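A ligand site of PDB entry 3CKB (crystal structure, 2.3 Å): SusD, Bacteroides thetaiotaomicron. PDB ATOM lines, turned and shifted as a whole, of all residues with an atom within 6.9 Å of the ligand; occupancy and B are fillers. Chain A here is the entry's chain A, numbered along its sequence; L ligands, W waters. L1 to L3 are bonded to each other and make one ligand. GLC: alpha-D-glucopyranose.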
ATOM      1  N   GLN A  48     -17.504 -25.552   3.635  1.00  0.00           N
ATOM      2  CA  GLN A  48     -18.384 -24.597   2.968  1.00  0.00           C
ATOM      3  C   GLN A  48     -19.741 -24.502   3.651  1.00  0.00           C
ATOM      4  O   GLN A  48     -20.389 -25.516   3.908  1.00  0.00           O
ATOM      5  CB  GLN A  48     -18.591 -24.989   1.501  1.00  0.00           C
ATOM      6  CG  GLN A  48     -17.404 -24.657   0.619  1.00  0.00           C
ATOM      7  CD  GLN A  48     -17.587 -25.136  -0.799  1.00  0.00           C
ATOM      8  OE1 GLN A  48     -16.805 -24.800  -1.702  1.00  0.00           O
ATOM      9  NE2 GLN A  48     -18.608 -25.948  -1.024  1.00  0.00           N
ATOM     10  N   ASP A  49     -20.163 -23.278   3.948  1.00  0.00           N
ATOM     11  CA  ASP A  49     -21.457 -23.056   4.583  1.00  0.00           C
ATOM     12  C   ASP A  49     -22.528 -23.160   3.497  1.00  0.00           C
ATOM     13  O   ASP A  49     -22.265 -23.670   2.403  1.00  0.00           O
ATOM     14  CB  ASP A  49     -21.485 -21.670   5.242  1.00  0.00           C
ATOM     15  CG  ASP A  49     -22.342 -21.639   6.495  1.00  0.00           C
ATOM     16  OD1 ASP A  49     -23.446 -22.236   6.495  1.00  0.00           O
ATOM     17  OD2 ASP A  49     -21.926 -21.000   7.485  1.00  0.00           O
ATOM     18  N   GLU A  50     -23.726 -22.667   3.784  1.00  0.00           N
ATOM     19  CA  GLU A  50     -24.822 -22.726   2.818  1.00  0.00           C
ATOM     20  C   GLU A  50     -24.567 -21.865   1.580  1.00  0.00           C
ATOM     21  O   GLU A  50     -24.375 -20.648   1.676  1.00  0.00           O
ATOM     22  CB  GLU A  50     -26.139 -22.295   3.460  1.00  0.00           C
ATOM     23  CG  GLU A  50     -26.438 -22.963   4.795  1.00  0.00           C
ATOM     24  CD  GLU A  50     -27.912 -22.859   5.189  1.00  0.00           C
ATOM     25  OE1 GLU A  50     -28.555 -21.827   4.874  1.00  0.00           O
ATOM     26  OE2 GLU A  50     -28.422 -23.807   5.819  1.00  0.00           O
ATOM     27  N   GLY A  51     -24.550 -22.520   0.424  1.00  0.00           N
ATOM     28  CA  GLY A  51     -24.362 -21.836  -0.846  1.00  0.00           C
ATOM     29  C   GLY A  51     -23.011 -21.211  -1.156  1.00  0.00           C
ATOM     30  O   GLY A  51     -22.914 -20.429  -2.109  1.00  0.00           O
ATOM     31  N   GLU A  52     -21.972 -21.549  -0.404  1.00  0.00           N
ATOM     32  CA  GLU A  52     -20.653 -20.973  -0.648  1.00  0.00           C
ATOM     33  C   GLU A  52     -19.952 -21.416  -1.935  1.00  0.00           C
ATOM     34  O   GLU A  52     -19.081 -20.698  -2.435  1.00  0.00           O
ATOM     35  CB  GLU A  52     -19.724 -21.249   0.534  1.00  0.00           C
ATOM     36  CG  GLU A  52     -20.142 -20.571   1.825  1.00  0.00           C
ATOM     37  CD  GLU A  52     -18.953 -20.079   2.612  1.00  0.00           C
ATOM     38  OE1 GLU A  52     -18.402 -19.013   2.257  1.00  0.00           O
ATOM     39  OE2 GLU A  52     -18.560 -20.765   3.585  1.00  0.00           O
ATOM     40  N   ARG A  57     -21.191 -16.313  -6.037  1.00  0.00           N
ATOM     41  CA  ARG A  57     -20.405 -15.883  -4.879  1.00  0.00           C
ATOM     42  C   ARG A  57     -18.901 -16.045  -5.089  1.00  0.00           C
ATOM     43  O   ARG A  57     -18.136 -15.094  -4.897  1.00  0.00           O
ATOM     44  CB  ARG A  57     -20.840 -16.651  -3.631  1.00  0.00           C
ATOM     45  CG  ARG A  57     -22.308 -16.442  -3.277  1.00  0.00           C
ATOM     46  CD  ARG A  57     -22.681 -17.095  -1.961  1.00  0.00           C
ATOM     47  NE  ARG A  57     -24.129 -17.116  -1.769  1.00  0.00           N
ATOM     48  CZ  ARG A  57     -24.735 -17.601  -0.692  1.00  0.00           C
ATOM     49  NH1 ARG A  57     -24.028 -18.097   0.319  1.00  0.00           N
ATOM     50  NH2 ARG A  57     -26.067 -17.584  -0.612  1.00  0.00           N
ATOM     51  N   TRP A  72     -14.460  -7.399   3.395  1.00  0.00           N
ATOM     52  CA  TRP A  72     -15.203  -8.410   4.122  1.00  0.00           C
ATOM     53  C   TRP A  72     -14.943  -8.099   5.598  1.00  0.00           C
ATOM     54  O   TRP A  72     -13.789  -7.988   6.017  1.00  0.00           O
ATOM     55  CB  TRP A  72     -14.691  -9.808   3.753  1.00  0.00           C
ATOM     56  CG  TRP A  72     -15.441 -10.931   4.383  1.00  0.00           C
ATOM     57  CD1 TRP A  72     -15.084 -11.638   5.494  1.00  0.00           C
ATOM     58  CD2 TRP A  72     -16.698 -11.474   3.945  1.00  0.00           C
ATOM     59  NE1 TRP A  72     -16.039 -12.596   5.771  1.00  0.00           N
ATOM     60  CE2 TRP A  72     -17.037 -12.512   4.841  1.00  0.00           C
ATOM     61  CE3 TRP A  72     -17.569 -11.177   2.891  1.00  0.00           C
ATOM     62  CZ2 TRP A  72     -18.202 -13.265   4.711  1.00  0.00           C
ATOM     63  CZ3 TRP A  72     -18.737 -11.929   2.751  1.00  0.00           C
ATOM     64  CH2 TRP A  72     -19.042 -12.961   3.657  1.00  0.00           C
ATOM     65  N   TRP A  74     -15.475  -9.882   8.398  1.00  0.00           N
ATOM     66  CA  TRP A  74     -14.948 -10.927   9.275  1.00  0.00           C
ATOM     67  C   TRP A  74     -13.612 -11.459   8.791  1.00  0.00           C
ATOM     68  O   TRP A  74     -13.532 -12.518   8.182  1.00  0.00           O
ATOM     69  CB  TRP A  74     -15.963 -12.060   9.381  1.00  0.00           C
ATOM     70  CG  TRP A  74     -17.315 -11.528   9.681  1.00  0.00           C
ATOM     71  CD1 TRP A  74     -18.271 -11.160   8.776  1.00  0.00           C
ATOM     72  CD2 TRP A  74     -17.832 -11.189  10.969  1.00  0.00           C
ATOM     73  NE1 TRP A  74     -19.345 -10.594   9.428  1.00  0.00           N
ATOM     74  CE2 TRP A  74     -19.109 -10.613  10.772  1.00  0.00           C
ATOM     75  CE3 TRP A  74     -17.335 -11.315  12.279  1.00  0.00           C
ATOM     76  CZ2 TRP A  74     -19.894 -10.155  11.843  1.00  0.00           C
ATOM     77  CZ3 TRP A  74     -18.121 -10.867  13.340  1.00  0.00           C
ATOM     78  CH2 TRP A  74     -19.388 -10.289  13.108  1.00  0.00           C
ATOM     79  N   LYS A  76     -11.416 -13.009  10.190  1.00  0.00           N
ATOM     80  CA  LYS A  76     -11.005 -14.289  10.748  1.00  0.00           C
ATOM     81  C   LYS A  76     -11.400 -15.467   9.854  1.00  0.00           C
ATOM     82  O   LYS A  76     -10.768 -16.518   9.890  1.00  0.00           O
ATOM     83  CB  LYS A  76     -11.571 -14.474  12.152  1.00  0.00           C
ATOM     84  CG  LYS A  76     -10.902 -13.587  13.196  1.00  0.00           C
ATOM     85  CD  LYS A  76     -11.622 -13.640  14.548  1.00  0.00           C
ATOM     86  CE  LYS A  76     -11.025 -12.624  15.524  1.00  0.00           C
ATOM     87  NZ  LYS A  76     -11.864 -12.466  16.754  1.00  0.00           N
ATOM     88  N   ASN A  77     -12.453 -15.285   9.051  1.00  0.00           N
ATOM     89  CA  ASN A  77     -12.900 -16.341   8.146  1.00  0.00           C
ATOM     90  C   ASN A  77     -11.685 -16.802   7.338  1.00  0.00           C
ATOM     91  O   ASN A  77     -10.810 -15.993   7.011  1.00  0.00           O
ATOM     92  CB  ASN A  77     -13.991 -15.826   7.190  1.00  0.00           C
ATOM     93  CG  ASN A  77     -15.333 -15.595   7.882  1.00  0.00           C
ATOM     94  OD1 ASN A  77     -16.309 -15.184   7.242  1.00  0.00           O
ATOM     95  ND2 ASN A  77     -15.390 -15.852   9.183  1.00  0.00           N
ATOM     96  N   ARG A  94     -10.454 -20.081  -1.361  1.00  0.00           N
ATOM     97  CA  ARG A  94     -11.389 -19.380  -2.239  1.00  0.00           C
ATOM     98  C   ARG A  94     -11.026 -19.526  -3.699  1.00  0.00           C
ATOM     99  O   ARG A  94     -11.902 -19.560  -4.566  1.00  0.00           O
ATOM    100  CB  ARG A  94     -11.469 -17.889  -1.863  1.00  0.00           C
ATOM    101  CG  ARG A  94     -11.938 -17.612  -0.440  1.00  0.00           C
ATOM    102  CD  ARG A  94     -13.074 -18.550  -0.045  1.00  0.00           C
ATOM    103  NE  ARG A  94     -13.505 -18.357   1.339  1.00  0.00           N
ATOM    104  CZ  ARG A  94     -14.277 -17.364   1.758  1.00  0.00           C
ATOM    105  NH1 ARG A  94     -14.718 -16.464   0.883  1.00  0.00           N
ATOM    106  NH2 ARG A  94     -14.596 -17.247   3.038  1.00  0.00           N
ATOM    107  N   ASN A 271     -31.998 -19.430   0.610  1.00  0.00           N
ATOM    108  CA  ASN A 271     -30.709 -19.026   1.150  1.00  0.00           C
ATOM    109  C   ASN A 271     -29.491 -19.456   0.340  1.00  0.00           C
ATOM    110  O   ASN A 271     -28.357 -19.143   0.702  1.00  0.00           O
ATOM    111  CB  ASN A 271     -30.598 -19.575   2.571  1.00  0.00           C
ATOM    112  CG  ASN A 271     -29.725 -18.723   3.459  1.00  0.00           C
ATOM    113  OD1 ASN A 271     -29.878 -17.509   3.516  1.00  0.00           O
ATOM    114  ND2 ASN A 271     -28.810 -19.365   4.182  1.00  0.00           N
ATOM    115  N   THR A 276     -28.987 -13.391  -2.439  1.00  0.00           N
ATOM    116  CA  THR A 276     -29.083 -13.555  -0.994  1.00  0.00           C
ATOM    117  C   THR A 276     -27.816 -12.962  -0.394  1.00  0.00           C
ATOM    118  O   THR A 276     -27.856 -12.187   0.574  1.00  0.00           O
ATOM    119  CB  THR A 276     -29.125 -15.044  -0.587  1.00  0.00           C
ATOM    120  OG1 THR A 276     -30.328 -15.646  -1.059  1.00  0.00           O
ATOM    121  CG2 THR A 276     -29.047 -15.182   0.918  1.00  0.00           C
ATOM    122  N   TYR A 277     -26.687 -13.353  -0.989  1.00  0.00           N
ATOM    123  CA  TYR A 277     -25.365 -12.909  -0.587  1.00  0.00           C
ATOM    124  C   TYR A 277     -25.255 -11.378  -0.725  1.00  0.00           C
ATOM    125  O   TYR A 277     -24.715 -10.701   0.141  1.00  0.00           O
ATOM    126  CB  TYR A 277     -24.331 -13.602  -1.483  1.00  0.00           C
ATOM    127  CG  TYR A 277     -22.882 -13.417  -1.097  1.00  0.00           C
ATOM    128  CD1 TYR A 277     -22.344 -14.094  -0.002  1.00  0.00           C
ATOM    129  CD2 TYR A 277     -22.040 -12.609  -1.855  1.00  0.00           C
ATOM    130  CE1 TYR A 277     -21.005 -13.962   0.338  1.00  0.00           C
ATOM    131  CE2 TYR A 277     -20.697 -12.465  -1.528  1.00  0.00           C
ATOM    132  CZ  TYR A 277     -20.182 -13.137  -0.436  1.00  0.00           C
ATOM    133  OH  TYR A 277     -18.854 -13.018  -0.103  1.00  0.00           O
ATOM    134  N   ASN A 294     -32.504 -11.094   8.047  1.00  0.00           N
ATOM    135  CA  ASN A 294     -31.167 -11.496   8.447  1.00  0.00           C
ATOM    136  C   ASN A 294     -30.033 -10.779   7.728  1.00  0.00           C
ATOM    137  O   ASN A 294     -29.682 -11.116   6.597  1.00  0.00           O
ATOM    138  CB  ASN A 294     -31.034 -13.010   8.287  1.00  0.00           C
ATOM    139  CG  ASN A 294     -29.664 -13.538   8.704  1.00  0.00           C
ATOM    140  OD1 ASN A 294     -28.955 -12.904   9.497  1.00  0.00           O
ATOM    141  ND2 ASN A 294     -29.297 -14.719   8.201  1.00  0.00           N
ATOM    142  N   GLY A 295     -29.475  -9.788   8.403  1.00  0.00           N
ATOM    143  CA  GLY A 295     -28.359  -9.046   7.846  1.00  0.00           C
ATOM    144  C   GLY A 295     -27.082  -9.688   8.362  1.00  0.00           C
ATOM    145  O   GLY A 295     -26.892  -9.797   9.567  1.00  0.00           O
ATOM    146  N   TRP A 296     -26.220 -10.122   7.444  1.00  0.00           N
ATOM    147  CA  TRP A 296     -24.968 -10.776   7.810  1.00  0.00           C
ATOM    148  C   TRP A 296     -23.857  -9.804   8.187  1.00  0.00           C
ATOM    149  O   TRP A 296     -22.861 -10.200   8.767  1.00  0.00           O
ATOM    150  CB  TRP A 296     -24.462 -11.642   6.659  1.00  0.00           C
ATOM    151  CG  TRP A 296     -25.431 -12.643   6.134  1.00  0.00           C
ATOM    152  CD1 TRP A 296     -26.652 -12.977   6.650  1.00  0.00           C
ATOM    153  CD2 TRP A 296     -25.251 -13.488   4.990  1.00  0.00           C
ATOM    154  NE1 TRP A 296     -27.236 -13.962   5.899  1.00  0.00           N
ATOM    155  CE2 TRP A 296     -26.397 -14.298   4.878  1.00  0.00           C
ATOM    156  CE3 TRP A 296     -24.216 -13.628   4.043  1.00  0.00           C
ATOM    157  CZ2 TRP A 296     -26.554 -15.237   3.854  1.00  0.00           C
ATOM    158  CZ3 TRP A 296     -24.370 -14.567   3.029  1.00  0.00           C
ATOM    159  CH2 TRP A 296     -25.533 -15.361   2.943  1.00  0.00           C
ATOM    160  N   SER A 297     -24.035  -8.528   7.849  1.00  0.00           N
ATOM    161  CA  SER A 297     -23.034  -7.506   8.121  1.00  0.00           C
ATOM    162  C   SER A 297     -21.645  -8.018   7.714  1.00  0.00           C
ATOM    163  O   SER A 297     -20.735  -8.109   8.535  1.00  0.00           O
ATOM    164  CB  SER A 297     -23.042  -7.090   9.602  1.00  0.00           C
ATOM    165  OG  SER A 297     -22.759  -8.187  10.453  1.00  0.00           O
ATOM    166  N   CYS A 298     -21.497  -8.345   6.426  1.00  0.00           N
ATOM    167  CA  CYS A 298     -20.251  -8.876   5.896  1.00  0.00           C
ATOM    168  C   CYS A 298     -19.553  -7.953   4.904  1.00  0.00           C
ATOM    169  O   CYS A 298     -18.331  -7.831   4.913  1.00  0.00           O
ATOM    170  CB  CYS A 298     -20.487 -10.206   5.190  1.00  0.00           C
ATOM    171  SG  CYS A 298     -20.974 -11.565   6.234  1.00  0.00           S
HETATM  172  C1  GLC L   1     -24.544 -18.582   5.543  1.00  0.00           C
HETATM  173  C2  GLC L   1     -23.391 -17.992   4.699  1.00  0.00           C
HETATM  174  C3  GLC L   1     -22.316 -17.538   5.702  1.00  0.00           C
HETATM  175  C4  GLC L   1     -22.921 -16.465   6.622  1.00  0.00           C
HETATM  176  C5  GLC L   1     -24.144 -17.100   7.353  1.00  0.00           C
HETATM  177  C6  GLC L   1     -24.799 -16.037   8.247  1.00  0.00           C
HETATM  178  O1  GLC L   1     -25.555 -19.158   4.715  1.00  0.00           O
HETATM  179  O2  GLC L   1     -22.835 -19.005   3.866  1.00  0.00           O
HETATM  180  O3  GLC L   1     -21.214 -16.961   4.991  1.00  0.00           O
HETATM  181  O4  GLC L   1     -21.921 -16.068   7.589  1.00  0.00           O
HETATM  182  O5  GLC L   1     -25.131 -17.555   6.386  1.00  0.00           O
HETATM  183  O6  GLC L   1     -25.859 -16.646   9.000  1.00  0.00           O
HETATM  184  C1  GLC L   2     -21.480 -14.691   7.440  1.00  0.00           C
HETATM  185  C2  GLC L   2     -19.971 -14.645   7.783  1.00  0.00           C
HETATM  186  C3  GLC L   2     -19.809 -15.204   9.221  1.00  0.00           C
HETATM  187  C4  GLC L   2     -20.599 -14.315  10.176  1.00  0.00           C
HETATM  188  C5  GLC L   2     -22.101 -14.328   9.745  1.00  0.00           C
HETATM  189  C6  GLC L   2     -22.941 -13.439  10.675  1.00  0.00           C
HETATM  190  O2  GLC L   2     -19.232 -15.485   6.872  1.00  0.00           O
HETATM  191  O3  GLC L   2     -18.424 -15.186   9.594  1.00  0.00           O
HETATM  192  O4  GLC L   2     -20.478 -14.841  11.510  1.00  0.00           O
HETATM  193  O5  GLC L   2     -22.227 -13.843   8.363  1.00  0.00           O
HETATM  194  O6  GLC L   2     -22.511 -12.075  10.582  1.00  0.00           O
HETATM  195  C1  GLC L   3     -19.906 -13.870  12.412  1.00  0.00           C
HETATM  196  C2  GLC L   3     -18.731 -14.507  13.211  1.00  0.00           C
HETATM  197  C3  GLC L   3     -19.284 -15.713  13.994  1.00  0.00           C
HETATM  198  C4  GLC L   3     -20.388 -15.209  14.942  1.00  0.00           C
HETATM  199  C5  GLC L   3     -21.496 -14.547  14.100  1.00  0.00           C
HETATM  200  C6  GLC L   3     -22.578 -14.008  15.040  1.00  0.00           C
HETATM  201  O2  GLC L   3     -17.701 -14.946  12.314  1.00  0.00           O
HETATM  202  O3  GLC L   3     -18.244 -16.338  14.751  1.00  0.00           O
HETATM  203  O4  GLC L   3     -20.932 -16.331  15.676  1.00  0.00           O
HETATM  204  O5  GLC L   3     -20.941 -13.413  13.341  1.00  0.00           O
HETATM  205  O6  GLC L   3     -23.822 -13.940  14.335  1.00  0.00           O
HETATM  206  O   HOH W   1     -28.703 -17.188  10.129  1.00  0.00           O
HETATM  207  O   HOH W   2     -26.533 -20.614   7.229  1.00  0.00           O
HETATM  208  O   HOH W   3     -27.789 -17.447   6.415  1.00  0.00           O
HETATM  209  O   HOH W   4     -26.172 -18.783   2.181  1.00  0.00           O
HETATM  210  O   HOH W   5     -22.299 -16.047  17.947  1.00  0.00           O
HETATM  211  O   HOH W   6     -21.536 -17.231   1.203  1.00  0.00           O
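OE2 of Glu 52 lies within hydrogen-bond range of N of Asp 49, 3.0 Å away.
The indole nitrogen (NE1) of Trp 74 lies within hydrogen-bond range of the side-chain sulfur (SG) of Cys 298, 3.7 Å away.
SG of Cys 298 is in hydrogen-bond range of O of Trp 296.
The side-chain carboxylate (OE1) of Glu 50 lies within hydrogen-bond range of the side-chain amide nitrogen (ND2) of Asn 271.
The indole nitrogen (NE1) of Trp 72 lies close to the backbone carbonyl oxygen (O) of Trp 74.
The backbone carbonyl oxygen of Ser 297 lies within hydrogen-bond range of the indole nitrogen of Trp 74, 3.0 Å away.
NH2 of Arg 57 is in hydrogen-bond range of O of Asn 271, 3.1 Å away.
The guanidinium group of Arg 57 sits at hydrogen-bond distance from the backbone carbonyl oxygen of Glu 50, 2.9 Å away.
O of Trp 296 sits at hydrogen-bond distance from O6 of GLC L2 (2.6 Å).
An oxygen (O1) of GLC L1 sits at hydrogen-bond distance from the side-chain amide nitrogen (ND2) of Asn 271.
The backbone carbonyl oxygen of Glu 50 sits at hydrogen-bond distance from an oxygen (O2) of GLC L1 (3.1 Å).
SG of Cys 298 sits at hydrogen-bond distance from O5 of GLC L2.
OD1 of Asn 77 is in hydrogen-bond range of O2 of GLC L2 (3.0 Å).
Water W4 lies within hydrogen-bond range of O1 of GLC L1, O of Glu 50, O of Asn 271 and NH1 of Arg 57.
Water W3 lies within hydrogen-bond range of O5 of GLC L1 and ND2 of Asn 271.
Water W2 lies within hydrogen-bond range of O1 of GLC L1 (3.1 Å) and OE1 of Glu 50 (3.3 Å).
Water W1 lies within hydrogen-bond range of an oxygen (O6) of GLC L1 (3.1 Å) and the side-chain amide nitrogen (ND2) of Asn 294 (3.2 Å).
Water W6 lies within hydrogen-bond range of the guanidinium group of Arg 57 (2.8 Å) and an oxygen (O2) of GLC L1 (3.5 Å).
CB of Asp 49 touches O2 of GLC L1 (3.3 Å).
CG of Glu 52 touches O2 of GLC L1 (3.7 Å).
NH1 of Arg 57 touches O2 of GLC L1, at 3.9 Å.
CZ2 of Trp 72 touches O2 of GLC L2, at 3.3 Å.
CZ2 of Trp 74 touches O6 of GLC L2, at 3.5 Å.
OG of Ser 297 touches O6 of GLC L2 (3.9 Å).
Hydrophobic or aromatic side chains that line the ligand: Trp 72, Trp 74 and Trp 296.
Within 4 Å of the ligand: Asp 49, Glu 50, Glu 52, Arg 57, Trp 72, Trp 74, Asn 77, Asn 271, Trp 296, Ser 297 and Cys 298.
The nearest printed residue that does not touch the ligand is Asn 294 (4.02 Å).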
